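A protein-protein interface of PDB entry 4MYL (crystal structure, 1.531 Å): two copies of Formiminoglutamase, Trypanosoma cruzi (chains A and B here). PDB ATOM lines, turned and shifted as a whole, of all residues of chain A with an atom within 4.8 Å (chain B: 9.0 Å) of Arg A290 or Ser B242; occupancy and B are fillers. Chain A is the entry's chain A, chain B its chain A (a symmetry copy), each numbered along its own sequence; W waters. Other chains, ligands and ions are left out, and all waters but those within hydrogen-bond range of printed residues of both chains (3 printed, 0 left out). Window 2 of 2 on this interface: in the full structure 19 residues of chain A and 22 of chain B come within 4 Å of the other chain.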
ATOM      1  N   SER A 243     -16.916  -8.011  16.113  1.00  0.00           N
ATOM      2  CA  SER A 243     -18.158  -7.567  16.759  1.00  0.00           C
ATOM      3  C   SER A 243     -18.299  -8.177  18.162  1.00  0.00           C
ATOM      4  O   SER A 243     -18.833  -7.537  19.078  1.00  0.00           O
ATOM      5  CB  SER A 243     -19.374  -7.919  15.912  1.00  0.00           C
ATOM      6  OG  SER A 243     -19.511  -9.320  15.787  1.00  0.00           O
ATOM      7  N   ASP A 244     -17.798  -9.411  18.311  1.00  0.00           N
ATOM      8  CA  ASP A 244     -17.807 -10.149  19.575  1.00  0.00           C
ATOM      9  C   ASP A 244     -16.492 -10.050  20.341  1.00  0.00           C
ATOM     10  O   ASP A 244     -16.474 -10.076  21.579  1.00  0.00           O
ATOM     11  CB  ASP A 244     -18.074 -11.632  19.322  1.00  0.00           C
ATOM     12  CG  ASP A 244     -19.401 -11.875  18.703  1.00  0.00           C
ATOM     13  OD1 ASP A 244     -20.021 -10.898  18.229  1.00  0.00           O
ATOM     14  OD2 ASP A 244     -19.816 -13.047  18.667  1.00  0.00           O
ATOM     15  N   PRO A 246     -13.351  -7.691  19.992  1.00  0.00           N
ATOM     16  CA  PRO A 246     -12.586  -6.597  19.366  1.00  0.00           C
ATOM     17  C   PRO A 246     -11.149  -6.492  19.878  1.00  0.00           C
ATOM     18  O   PRO A 246     -10.279  -6.033  19.131  1.00  0.00           O
ATOM     19  CB  PRO A 246     -13.377  -5.329  19.720  1.00  0.00           C
ATOM     20  CG  PRO A 246     -14.437  -5.730  20.691  1.00  0.00           C
ATOM     21  CD  PRO A 246     -14.371  -7.209  20.943  1.00  0.00           C
ATOM     22  N   GLU A 287      -8.978  -3.471  23.275  1.00  0.00           N
ATOM     23  CA  GLU A 287     -10.236  -3.357  24.022  1.00  0.00           C
ATOM     24  C   GLU A 287     -10.142  -4.174  25.319  1.00  0.00           C
ATOM     25  O   GLU A 287      -9.743  -5.339  25.293  1.00  0.00           O
ATOM     26  CB  GLU A 287     -11.418  -3.796  23.159  1.00  0.00           C
ATOM     27  CG  GLU A 287     -12.781  -3.420  23.718  1.00  0.00           C
ATOM     28  CD  GLU A 287     -13.276  -4.414  24.748  1.00  0.00           C
ATOM     29  OE1 GLU A 287     -12.933  -5.611  24.597  1.00  0.00           O
ATOM     30  OE2 GLU A 287     -14.015  -4.011  25.680  1.00  0.00           O
ATOM     31  N   GLU A 288     -10.491  -3.569  26.454  1.00  0.00           N
ATOM     32  CA  GLU A 288     -10.115  -4.142  27.743  1.00  0.00           C
ATOM     33  C   GLU A 288     -11.228  -4.736  28.588  1.00  0.00           C
ATOM     34  O   GLU A 288     -10.951  -5.327  29.631  1.00  0.00           O
ATOM     35  CB  GLU A 288      -9.399  -3.094  28.586  1.00  0.00           C
ATOM     36  CG  GLU A 288     -10.302  -2.018  29.152  1.00  0.00           C
ATOM     37  CD  GLU A 288      -9.562  -1.107  30.124  1.00  0.00           C
ATOM     38  OE1 GLU A 288      -9.632   0.121  29.938  1.00  0.00           O
ATOM     39  OE2 GLU A 288      -8.903  -1.616  31.060  1.00  0.00           O
ATOM     40  N   TYR A 289     -12.478  -4.564  28.168  1.00  0.00           N
ATOM     41  CA  TYR A 289     -13.616  -4.990  28.989  1.00  0.00           C
ATOM     42  C   TYR A 289     -14.280  -6.257  28.453  1.00  0.00           C
ATOM     43  O   TYR A 289     -14.245  -7.306  29.090  1.00  0.00           O
ATOM     44  CB  TYR A 289     -14.645  -3.855  29.122  1.00  0.00           C
ATOM     45  CG  TYR A 289     -14.071  -2.568  29.709  1.00  0.00           C
ATOM     46  CD1 TYR A 289     -13.897  -1.436  28.920  1.00  0.00           C
ATOM     47  CD2 TYR A 289     -13.687  -2.494  31.048  1.00  0.00           C
ATOM     48  CE1 TYR A 289     -13.363  -0.262  29.446  1.00  0.00           C
ATOM     49  CE2 TYR A 289     -13.151  -1.322  31.584  1.00  0.00           C
ATOM     50  CZ  TYR A 289     -12.995  -0.213  30.777  1.00  0.00           C
ATOM     51  OH  TYR A 289     -12.472   0.950  31.295  1.00  0.00           O
ATOM     52  N   ARG A 290     -14.862  -6.159  27.264  1.00  0.00           N
ATOM     53  CA  ARG A 290     -15.651  -7.255  26.710  1.00  0.00           C
ATOM     54  C   ARG A 290     -14.791  -8.443  26.321  1.00  0.00           C
ATOM     55  O   ARG A 290     -15.171  -9.602  26.529  1.00  0.00           O
ATOM     56  CB  ARG A 290     -16.446  -6.765  25.496  1.00  0.00           C
ATOM     57  CG  ARG A 290     -17.490  -5.674  25.830  1.00  0.00           C
ATOM     58  CD  ARG A 290     -18.069  -5.072  24.582  1.00  0.00           C
ATOM     59  NE  ARG A 290     -18.628  -6.123  23.744  1.00  0.00           N
ATOM     60  CZ  ARG A 290     -18.417  -6.267  22.436  1.00  0.00           C
ATOM     61  NH1 ARG A 290     -17.665  -5.404  21.771  1.00  0.00           N
ATOM     62  NH2 ARG A 290     -18.986  -7.279  21.785  1.00  0.00           N
ATOM     63  N   SER A 291     -13.629  -8.157  25.745  1.00  0.00           N
ATOM     64  CA  SER A 291     -12.806  -9.217  25.153  1.00  0.00           C
ATOM     65  C   SER A 291     -12.166 -10.171  26.181  1.00  0.00           C
ATOM     66  O   SER A 291     -12.189 -11.387  26.002  1.00  0.00           O
ATOM     67  CB  SER A 291     -11.784  -8.633  24.171  1.00  0.00           C
ATOM     68  OG  SER A 291     -12.457  -7.850  23.199  1.00  0.00           O
ATOM     69  N   PRO A 292     -11.615  -9.625  27.274  1.00  0.00           N
ATOM     70  CA  PRO A 292     -11.107 -10.538  28.304  1.00  0.00           C
ATOM     71  C   PRO A 292     -12.209 -11.392  28.934  1.00  0.00           C
ATOM     72  O   PRO A 292     -11.938 -12.528  29.329  1.00  0.00           O
ATOM     73  CB  PRO A 292     -10.481  -9.582  29.325  1.00  0.00           C
ATOM     74  CG  PRO A 292     -10.066  -8.393  28.492  1.00  0.00           C
ATOM     75  CD  PRO A 292     -11.195  -8.233  27.518  1.00  0.00           C
ATOM     76  N   ARG A 293     -13.434 -10.871  29.015  1.00  0.00           N
ATOM     77  CA  ARG A 293     -14.565 -11.692  29.471  1.00  0.00           C
ATOM     78  C   ARG A 293     -14.816 -12.873  28.519  1.00  0.00           C
ATOM     79  O   ARG A 293     -14.997 -14.007  28.940  1.00  0.00           O
ATOM     80  CB  ARG A 293     -15.833 -10.848  29.643  1.00  0.00           C
ATOM     81  CG  ARG A 293     -15.725  -9.826  30.784  1.00  0.00           C
ATOM     82  CD  ARG A 293     -17.009  -8.992  30.975  1.00  0.00           C
ATOM     83  NE  ARG A 293     -18.130  -9.825  31.388  1.00  0.00           N
ATOM     84  CZ  ARG A 293     -18.668  -9.818  32.605  1.00  0.00           C
ATOM     85  NH1 ARG A 293     -18.192  -9.008  33.539  1.00  0.00           N
ATOM     86  NH2 ARG A 293     -19.688 -10.619  32.884  1.00  0.00           N
ATOM     87  N   VAL A 294     -14.818 -12.601  27.219  1.00  0.00           N
ATOM     88  CA  VAL A 294     -14.987 -13.669  26.246  1.00  0.00           C
ATOM     89  C   VAL A 294     -13.882 -14.713  26.435  1.00  0.00           C
ATOM     90  O   VAL A 294     -14.156 -15.907  26.435  1.00  0.00           O
ATOM     91  CB  VAL A 294     -14.987 -13.136  24.800  1.00  0.00           C
ATOM     92  CG1 VAL A 294     -14.976 -14.297  23.788  1.00  0.00           C
ATOM     93  CG2 VAL A 294     -16.194 -12.210  24.563  1.00  0.00           C
ATOM     94  N   ARG B  49     -21.786  -2.279  36.480  1.00  0.00           N
ATOM     95  CA  ARG B  49     -21.331  -0.896  36.518  1.00  0.00           C
ATOM     96  C   ARG B  49     -22.457   0.044  36.909  1.00  0.00           C
ATOM     97  O   ARG B  49     -23.610  -0.161  36.532  1.00  0.00           O
ATOM     98  CB  ARG B  49     -20.739  -0.475  35.162  1.00  0.00           C
ATOM     99  CG  ARG B  49     -19.481  -1.252  34.769  1.00  0.00           C
ATOM    100  CD  ARG B  49     -18.411  -0.343  34.176  1.00  0.00           C
ATOM    101  NE  ARG B  49     -17.967  -0.832  32.872  1.00  0.00           N
ATOM    102  CZ  ARG B  49     -17.560  -0.054  31.869  1.00  0.00           C
ATOM    103  NH1 ARG B  49     -17.533   1.266  32.014  1.00  0.00           N
ATOM    104  NH2 ARG B  49     -17.188  -0.598  30.715  1.00  0.00           N
ATOM    105  N   GLN B 186     -28.772 -17.326  31.502  1.00  0.00           N
ATOM    106  CA  GLN B 186     -27.509 -17.923  31.076  1.00  0.00           C
ATOM    107  C   GLN B 186     -26.876 -18.751  32.200  1.00  0.00           C
ATOM    108  O   GLN B 186     -26.609 -18.219  33.275  1.00  0.00           O
ATOM    109  CB  GLN B 186     -26.551 -16.821  30.620  1.00  0.00           C
ATOM    110  CG  GLN B 186     -27.032 -16.099  29.386  1.00  0.00           C
ATOM    111  CD  GLN B 186     -26.086 -14.998  28.942  1.00  0.00           C
ATOM    112  OE1 GLN B 186     -24.933 -14.944  29.367  1.00  0.00           O
ATOM    113  NE2 GLN B 186     -26.574 -14.116  28.080  1.00  0.00           N
ATOM    114  N   VAL B 237     -32.207  -5.458  29.757  1.00  0.00           N
ATOM    115  CA  VAL B 237     -31.404  -5.434  28.547  1.00  0.00           C
ATOM    116  C   VAL B 237     -30.054  -6.147  28.724  1.00  0.00           C
ATOM    117  O   VAL B 237     -29.291  -6.303  27.758  1.00  0.00           O
ATOM    118  CB  VAL B 237     -31.240  -4.002  27.964  1.00  0.00           C
ATOM    119  CG1 VAL B 237     -32.573  -3.510  27.434  1.00  0.00           C
ATOM    120  CG2 VAL B 237     -30.671  -3.034  28.984  1.00  0.00           C
ATOM    121  N   ASP B 238     -29.766  -6.571  29.957  1.00  0.00           N
ATOM    122  CA  ASP B 238     -28.596  -7.407  30.225  1.00  0.00           C
ATOM    123  C   ASP B 238     -28.677  -8.729  29.454  1.00  0.00           C
ATOM    124  O   ASP B 238     -27.669  -9.438  29.283  1.00  0.00           O
ATOM    125  CB  ASP B 238     -28.449  -7.691  31.726  1.00  0.00           C
ATOM    126  CG  ASP B 238     -27.852  -6.511  32.510  1.00  0.00           C
ATOM    127  OD1 ASP B 238     -27.913  -6.557  33.759  1.00  0.00           O
ATOM    128  OD2 ASP B 238     -27.328  -5.549  31.901  1.00  0.00           O
ATOM    129  N   SER B 239     -29.884  -9.053  28.991  1.00  0.00           N
ATOM    130  CA  SER B 239     -30.139 -10.289  28.242  1.00  0.00           C
ATOM    131  C   SER B 239     -29.671 -10.242  26.780  1.00  0.00           C
ATOM    132  O   SER B 239     -29.637 -11.276  26.123  1.00  0.00           O
ATOM    133  CB  SER B 239     -31.622 -10.651  28.283  1.00  0.00           C
ATOM    134  OG  SER B 239     -32.391  -9.677  27.615  1.00  0.00           O
ATOM    135  N   LEU B 240     -29.345  -9.051  26.271  1.00  0.00           N
ATOM    136  CA  LEU B 240     -28.855  -8.909  24.891  1.00  0.00           C
ATOM    137  C   LEU B 240     -27.349  -9.094  24.826  1.00  0.00           C
ATOM    138  O   LEU B 240     -26.637  -8.761  25.754  1.00  0.00           O
ATOM    139  CB  LEU B 240     -29.241  -7.551  24.270  1.00  0.00           C
ATOM    140  CG  LEU B 240     -30.680  -7.397  23.760  1.00  0.00           C
ATOM    141  CD1 LEU B 240     -31.639  -7.184  24.910  1.00  0.00           C
ATOM    142  CD2 LEU B 240     -30.790  -6.257  22.742  1.00  0.00           C
ATOM    143  N   LYS B 241     -26.868  -9.618  23.711  1.00  0.00           N
ATOM    144  CA  LYS B 241     -25.432  -9.792  23.511  1.00  0.00           C
ATOM    145  C   LYS B 241     -24.766  -8.425  23.356  1.00  0.00           C
ATOM    146  O   LYS B 241     -25.331  -7.503  22.769  1.00  0.00           O
ATOM    147  CB  LYS B 241     -25.159 -10.689  22.300  1.00  0.00           C
ATOM    148  CG  LYS B 241     -25.640 -10.130  20.988  1.00  0.00           C
ATOM    149  CD  LYS B 241     -25.218 -11.029  19.826  1.00  0.00           C
ATOM    150  CE  LYS B 241     -26.202 -12.151  19.609  1.00  0.00           C
ATOM    151  NZ  LYS B 241     -25.886 -12.943  18.374  1.00  0.00           N
ATOM    152  N   SER B 242     -23.563  -8.290  23.892  1.00  0.00           N
ATOM    153  CA  SER B 242     -22.931  -6.977  23.937  1.00  0.00           C
ATOM    154  C   SER B 242     -22.425  -6.477  22.576  1.00  0.00           C
ATOM    155  O   SER B 242     -22.113  -5.304  22.438  1.00  0.00           O
ATOM    156  CB  SER B 242     -21.821  -6.915  25.001  1.00  0.00           C
ATOM    157  OG  SER B 242     -20.766  -7.817  24.716  1.00  0.00           O
ATOM    158  N   SER B 243     -22.369  -7.342  21.572  1.00  0.00           N
ATOM    159  CA  SER B 243     -22.037  -6.875  20.219  1.00  0.00           C
ATOM    160  C   SER B 243     -23.109  -5.911  19.690  1.00  0.00           C
ATOM    161  O   SER B 243     -22.799  -4.964  18.954  1.00  0.00           O
ATOM    162  CB  SER B 243     -21.868  -8.046  19.261  1.00  0.00           C
ATOM    163  OG  SER B 243     -23.082  -8.754  19.113  1.00  0.00           O
ATOM    164  N   ASP B 244     -24.363  -6.163  20.090  1.00  0.00           N
ATOM    165  CA  ASP B 244     -25.518  -5.343  19.720  1.00  0.00           C
ATOM    166  C   ASP B 244     -25.901  -4.323  20.786  1.00  0.00           C
ATOM    167  O   ASP B 244     -26.399  -3.232  20.474  1.00  0.00           O
ATOM    168  CB  ASP B 244     -26.741  -6.226  19.477  1.00  0.00           C
ATOM    169  CG  ASP B 244     -26.545  -7.178  18.355  1.00  0.00           C
ATOM    170  OD1 ASP B 244     -25.385  -7.345  17.918  1.00  0.00           O
ATOM    171  OD2 ASP B 244     -27.544  -7.778  17.924  1.00  0.00           O
ATOM    172  N   MET B 245     -25.692  -4.696  22.042  1.00  0.00           N
ATOM    173  CA  MET B 245     -26.164  -3.910  23.175  1.00  0.00           C
ATOM    174  C   MET B 245     -25.088  -3.781  24.251  1.00  0.00           C
ATOM    175  O   MET B 245     -25.190  -4.412  25.306  1.00  0.00           O
ATOM    176  CB  MET B 245     -27.386  -4.597  23.765  1.00  0.00           C
ATOM    177  CG  MET B 245     -28.133  -3.769  24.778  1.00  0.00           C
ATOM    178  SD  MET B 245     -28.806  -2.313  23.975  1.00  0.00           S
ATOM    179  CE  MET B 245     -30.171  -1.947  25.079  1.00  0.00           C
ATOM    180  N   PRO B 246     -24.046  -2.959  23.988  1.00  0.00           N
ATOM    181  CA  PRO B 246     -22.913  -2.897  24.930  1.00  0.00           C
ATOM    182  C   PRO B 246     -23.211  -2.070  26.181  1.00  0.00           C
ATOM    183  O   PRO B 246     -22.627  -2.347  27.234  1.00  0.00           O
ATOM    184  CB  PRO B 246     -21.779  -2.253  24.118  1.00  0.00           C
ATOM    185  CG  PRO B 246     -22.369  -1.797  22.824  1.00  0.00           C
ATOM    186  CD  PRO B 246     -23.827  -2.156  22.769  1.00  0.00           C
ATOM    187  N   GLY B 247     -24.113  -1.098  26.076  1.00  0.00           N
ATOM    188  CA  GLY B 247     -24.296  -0.118  27.131  1.00  0.00           C
ATOM    189  C   GLY B 247     -25.330  -0.532  28.151  1.00  0.00           C
ATOM    190  O   GLY B 247     -26.406   0.040  28.218  1.00  0.00           O
ATOM    191  N   VAL B 248     -24.992  -1.547  28.934  1.00  0.00           N
ATOM    192  CA  VAL B 248     -25.876  -2.089  29.953  1.00  0.00           C
ATOM    193  C   VAL B 248     -25.013  -2.335  31.190  1.00  0.00           C
ATOM    194  O   VAL B 248     -23.785  -2.338  31.105  1.00  0.00           O
ATOM    195  CB  VAL B 248     -26.584  -3.398  29.478  1.00  0.00           C
ATOM    196  CG1 VAL B 248     -27.348  -3.144  28.189  1.00  0.00           C
ATOM    197  CG2 VAL B 248     -25.594  -4.544  29.290  1.00  0.00           C
ATOM    198  N   CYS B 250     -24.624  -4.980  33.134  1.00  0.00           N
ATOM    199  CA  CYS B 250     -23.996  -6.291  33.181  1.00  0.00           C
ATOM    200  C   CYS B 250     -23.958  -6.889  31.782  1.00  0.00           C
ATOM    201  O   CYS B 250     -24.789  -7.726  31.447  1.00  0.00           O
ATOM    202  CB  CYS B 250     -24.759  -7.225  34.121  1.00  0.00           C
ATOM    203  SG  CYS B 250     -24.550  -6.855  35.903  1.00  0.00           S
ATOM    204  N   PRO B 251     -23.005  -6.432  30.953  1.00  0.00           N
ATOM    205  CA  PRO B 251     -22.901  -6.861  29.555  1.00  0.00           C
ATOM    206  C   PRO B 251     -22.675  -8.352  29.417  1.00  0.00           C
ATOM    207  O   PRO B 251     -22.055  -8.983  30.286  1.00  0.00           O
ATOM    208  CB  PRO B 251     -21.685  -6.093  29.042  1.00  0.00           C
ATOM    209  CG  PRO B 251     -21.619  -4.875  29.905  1.00  0.00           C
ATOM    210  CD  PRO B 251     -22.089  -5.316  31.259  1.00  0.00           C
ATOM    211  N   ALA B 252     -23.190  -8.900  28.320  1.00  0.00           N
ATOM    212  CA  ALA B 252     -23.145 -10.329  28.059  1.00  0.00           C
ATOM    213  C   ALA B 252     -22.340 -10.602  26.800  1.00  0.00           C
ATOM    214  O   ALA B 252     -22.431  -9.857  25.826  1.00  0.00           O
ATOM    215  CB  ALA B 252     -24.567 -10.884  27.902  1.00  0.00           C
ATOM    216  N   ALA B 253     -21.560 -11.680  26.827  1.00  0.00           N
ATOM    217  CA  ALA B 253     -20.799 -12.125  25.663  1.00  0.00           C
ATOM    218  C   ALA B 253     -21.737 -12.718  24.617  1.00  0.00           C
ATOM    219  O   ALA B 253     -21.665 -12.392  23.433  1.00  0.00           O
ATOM    220  CB  ALA B 253     -19.734 -13.147  26.083  1.00  0.00           C
ATOM    221  N   VAL B 254     -22.617 -13.605  25.074  1.00  0.00           N
ATOM    222  CA  VAL B 254     -23.682 -14.137  24.246  1.00  0.00           C
ATOM    223  C   VAL B 254     -25.019 -13.625  24.825  1.00  0.00           C
ATOM    224  O   VAL B 254     -25.062 -13.091  25.936  1.00  0.00           O
ATOM    225  CB  VAL B 254     -23.652 -15.654  24.216  1.00  0.00           C
ATOM    226  CG1 VAL B 254     -22.457 -16.148  23.408  1.00  0.00           C
ATOM    227  CG2 VAL B 254     -23.606 -16.197  25.640  1.00  0.00           C
ATOM    228  N   GLY B 255     -26.096 -13.765  24.064  1.00  0.00           N
ATOM    229  CA  GLY B 255     -27.372 -13.222  24.483  1.00  0.00           C
ATOM    230  C   GLY B 255     -28.242 -12.920  23.289  1.00  0.00           C
ATOM    231  O   GLY B 255     -27.882 -13.234  22.150  1.00  0.00           O
ATOM    232  N   LEU B 256     -29.399 -12.320  23.545  1.00  0.00           N
ATOM    233  CA  LEU B 256     -30.362 -12.055  22.484  1.00  0.00           C
ATOM    234  C   LEU B 256     -29.801 -11.039  21.492  1.00  0.00           C
ATOM    235  O   LEU B 256     -29.128 -10.090  21.883  1.00  0.00           O
ATOM    236  CB  LEU B 256     -31.675 -11.549  23.081  1.00  0.00           C
ATOM    237  CG  LEU B 256     -32.420 -12.511  24.015  1.00  0.00           C
ATOM    238  CD1 LEU B 256     -33.554 -11.800  24.707  1.00  0.00           C
ATOM    239  CD2 LEU B 256     -32.939 -13.721  23.230  1.00  0.00           C
ATOM    240  N   SER B 257     -30.085 -11.219  20.209  1.00  0.00           N
ATOM    241  CA  SER B 257     -29.690 -10.220  19.220  1.00  0.00           C
ATOM    242  C   SER B 257     -30.658  -9.035  19.254  1.00  0.00           C
ATOM    243  O   SER B 257     -31.760  -9.135  19.809  1.00  0.00           O
ATOM    244  CB  SER B 257     -29.666 -10.827  17.819  1.00  0.00           C
ATOM    245  OG  SER B 257     -30.989 -11.096  17.388  1.00  0.00           O
ATOM    246  N   ALA B 258     -30.256  -7.916  18.652  1.00  0.00           N
ATOM    247  CA  ALA B 258     -31.153  -6.776  18.543  1.00  0.00           C
ATOM    248  C   ALA B 258     -32.447  -7.177  17.807  1.00  0.00           C
ATOM    249  O   ALA B 258     -33.545  -6.857  18.264  1.00  0.00           O
ATOM    250  CB  ALA B 258     -30.452  -5.586  17.865  1.00  0.00           C
ATOM    251  N   VAL B 286     -21.751   3.145  30.287  1.00  0.00           N
ATOM    252  CA  VAL B 286     -21.016   2.074  29.625  1.00  0.00           C
ATOM    253  C   VAL B 286     -20.920   2.323  28.113  1.00  0.00           C
ATOM    254  O   VAL B 286     -19.835   2.214  27.537  1.00  0.00           O
ATOM    255  CB  VAL B 286     -21.602   0.692  29.931  1.00  0.00           C
ATOM    256  CG1 VAL B 286     -20.817  -0.377  29.206  1.00  0.00           C
ATOM    257  CG2 VAL B 286     -21.586   0.452  31.438  1.00  0.00           C
ATOM    258  N   GLU B 287     -22.043   2.656  27.476  1.00  0.00           N
ATOM    259  CA  GLU B 287     -22.049   3.074  26.070  1.00  0.00           C
ATOM    260  C   GLU B 287     -23.304   3.915  25.789  1.00  0.00           C
ATOM    261  O   GLU B 287     -24.413   3.514  26.139  1.00  0.00           O
ATOM    262  CB  GLU B 287     -21.958   1.862  25.146  1.00  0.00           C
ATOM    263  CG  GLU B 287     -21.640   2.196  23.697  1.00  0.00           C
ATOM    264  CD  GLU B 287     -22.872   2.594  22.912  1.00  0.00           C
ATOM    265  OE1 GLU B 287     -23.956   2.055  23.240  1.00  0.00           O
ATOM    266  OE2 GLU B 287     -22.756   3.411  21.966  1.00  0.00           O
ATOM    267  N   ARG B 290     -25.207   3.753  20.655  1.00  0.00           N
ATOM    268  CA  ARG B 290     -25.888   2.639  20.003  1.00  0.00           C
ATOM    269  C   ARG B 290     -26.946   2.013  20.893  1.00  0.00           C
ATOM    270  O   ARG B 290     -28.031   1.641  20.432  1.00  0.00           O
ATOM    271  CB  ARG B 290     -24.868   1.580  19.577  1.00  0.00           C
ATOM    272  CG  ARG B 290     -23.853   2.076  18.520  1.00  0.00           C
ATOM    273  CD  ARG B 290     -22.748   1.082  18.315  1.00  0.00           C
ATOM    274  NE  ARG B 290     -23.312  -0.213  17.962  1.00  0.00           N
ATOM    275  CZ  ARG B 290     -22.976  -1.382  18.508  1.00  0.00           C
ATOM    276  NH1 ARG B 290     -22.036  -1.450  19.439  1.00  0.00           N
ATOM    277  NH2 ARG B 290     -23.574  -2.498  18.097  1.00  0.00           N
ATOM    278  N   SER B 291     -26.625   1.884  22.176  1.00  0.00           N
ATOM    279  CA  SER B 291     -27.482   1.121  23.089  1.00  0.00           C
ATOM    280  C   SER B 291     -28.834   1.793  23.399  1.00  0.00           C
ATOM    281  O   SER B 291     -29.875   1.138  23.383  1.00  0.00           O
ATOM    282  CB  SER B 291     -26.716   0.722  24.355  1.00  0.00           C
ATOM    283  OG  SER B 291     -25.536   0.022  23.993  1.00  0.00           O
ATOM    284  N   VAL B 294     -31.084   1.123  20.484  1.00  0.00           N
ATOM    285  CA  VAL B 294     -31.667  -0.209  20.542  1.00  0.00           C
ATOM    286  C   VAL B 294     -32.846  -0.209  21.519  1.00  0.00           C
ATOM    287  O   VAL B 294     -33.900  -0.754  21.215  1.00  0.00           O
ATOM    288  CB  VAL B 294     -30.630  -1.274  20.945  1.00  0.00           C
ATOM    289  CG1 VAL B 294     -31.307  -2.637  21.183  1.00  0.00           C
ATOM    290  CG2 VAL B 294     -29.526  -1.388  19.878  1.00  0.00           C
HETATM  291  O   HOH W   1     -18.669  -9.787  23.251  1.00  0.00           O
HETATM  292  O   HOH W   2     -19.578  -4.367  18.500  1.00  0.00           O
HETATM  293  O   HOH W   3     -22.358 -13.017  20.825  1.00  0.00           O
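OG of Ser B242 is in hydrogen-bond range of NE of Arg A290 (2.9 Å). N of Ser B243 sits close to NH2 of Arg A290, at 3.4 Å.
The side-chain carboxylate (OD1) of Asp B244 lies within hydrogen-bond range of the side-chain hydroxyl (OG) of Ser B243, at 3.0 Å. The side-chain carboxylate (OE1) of Glu A288 sits at hydrogen-bond distance from the side-chain hydroxyl (OH) of Tyr A289. The backbone carbonyl oxygen (O) of Ser A243 sits at hydrogen-bond distance from the guanidinium group (NH2) of Arg A290 (2.7 Å). The side-chain hydroxyl of Ser A243 lies within hydrogen-bond range of the side-chain carboxylate of Asp A244 (3.0 Å). OE2 of Glu A287 lies within hydrogen-bond range of N of Tyr A289, at 3.0 Å. O of Ser B243 lies within hydrogen-bond range of NH2 of Arg B290 (2.7 Å).
Among the printed residues, merely in contact across the chains: Ser A243 with Ser B243 (3.1 Å), Asp A244 with Ser B243 (3.6 Å), Tyr A289 with Arg B49 (3.8 Å), Arg A293 with Pro B251 (3.9 Å) and Val A294 with Ala B253 (3.96 Å).
Of the printed residues of chain B, Ser A243 touches Ser B243 (3.1 Å). Printed residues of chain B within 4 Å of Asp A244: Ser B243 (3.6 Å). Of the printed residues of chain B, Tyr A289 touches Arg B49. Of chain B, only Ser B242 (2.9 Å) and Ser B243 (3.4 Å) come within 4 Å of Arg A290. Ser A291 touches none of the printed residues of chain B. Pro A292 touches none of the printed residues of chain B. Ser B242 touches just one residue of chain A: Arg A290. Printed residues of chain A within 4 Å of Ser B243: Ser A243, Asp A244 and Arg A290. Of the printed residues of chain A, Pro B251 touches Arg A293 (3.9 Å). The nearest residue of chain B that does not touch Arg A290 is Pro B246 (4.7 Å). The nearest printed residue of chain A that does not touch Ser B242 is Ser A243 (5.1 Å).
Hydrophobic or aromatic side chains of chain A that line the printed part of chain B: Tyr A289 and Val A294. Along chain A the printed residues that touch a printed residue of chain B span positions 243 to 294. Of the 28 printed residues of chain B, 5 touch a printed residue of chain A. Hydrophobic or aromatic side chains of chain B that line the printed part of chain A: Ala B253. Among the printed residues, no Asp or Glu carboxylate lies within 4 Å of a Lys or Arg side-chain nitrogen of the other chain.
Ser A243 touches its own counterpart, Ser B243. Asp A244 touches Ser B243, but with the chains exchanged Ser A243 does not touch Asp B244 (5.8 Å). Arg A290 touches Ser B243, but with the chains exchanged Ser A243 does not touch Arg B290 (6.9 Å).
Water W3 bridges the backbone carbonyl oxygen (O) of Ala B253 (2.8 Å) and the side-chain carboxylate (OD2) of Asp A244 (3.3 Å). Water W1 lies within hydrogen-bond range of O of Asp A244 (2.8 Å), NH2 of Arg A290 (2.9 Å) and OG of Ser B242 (3.2 Å). Water W2 lies within hydrogen-bond range of the backbone carbonyl oxygen of Ser B243 and the backbone carbonyl oxygen of Ser A243.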
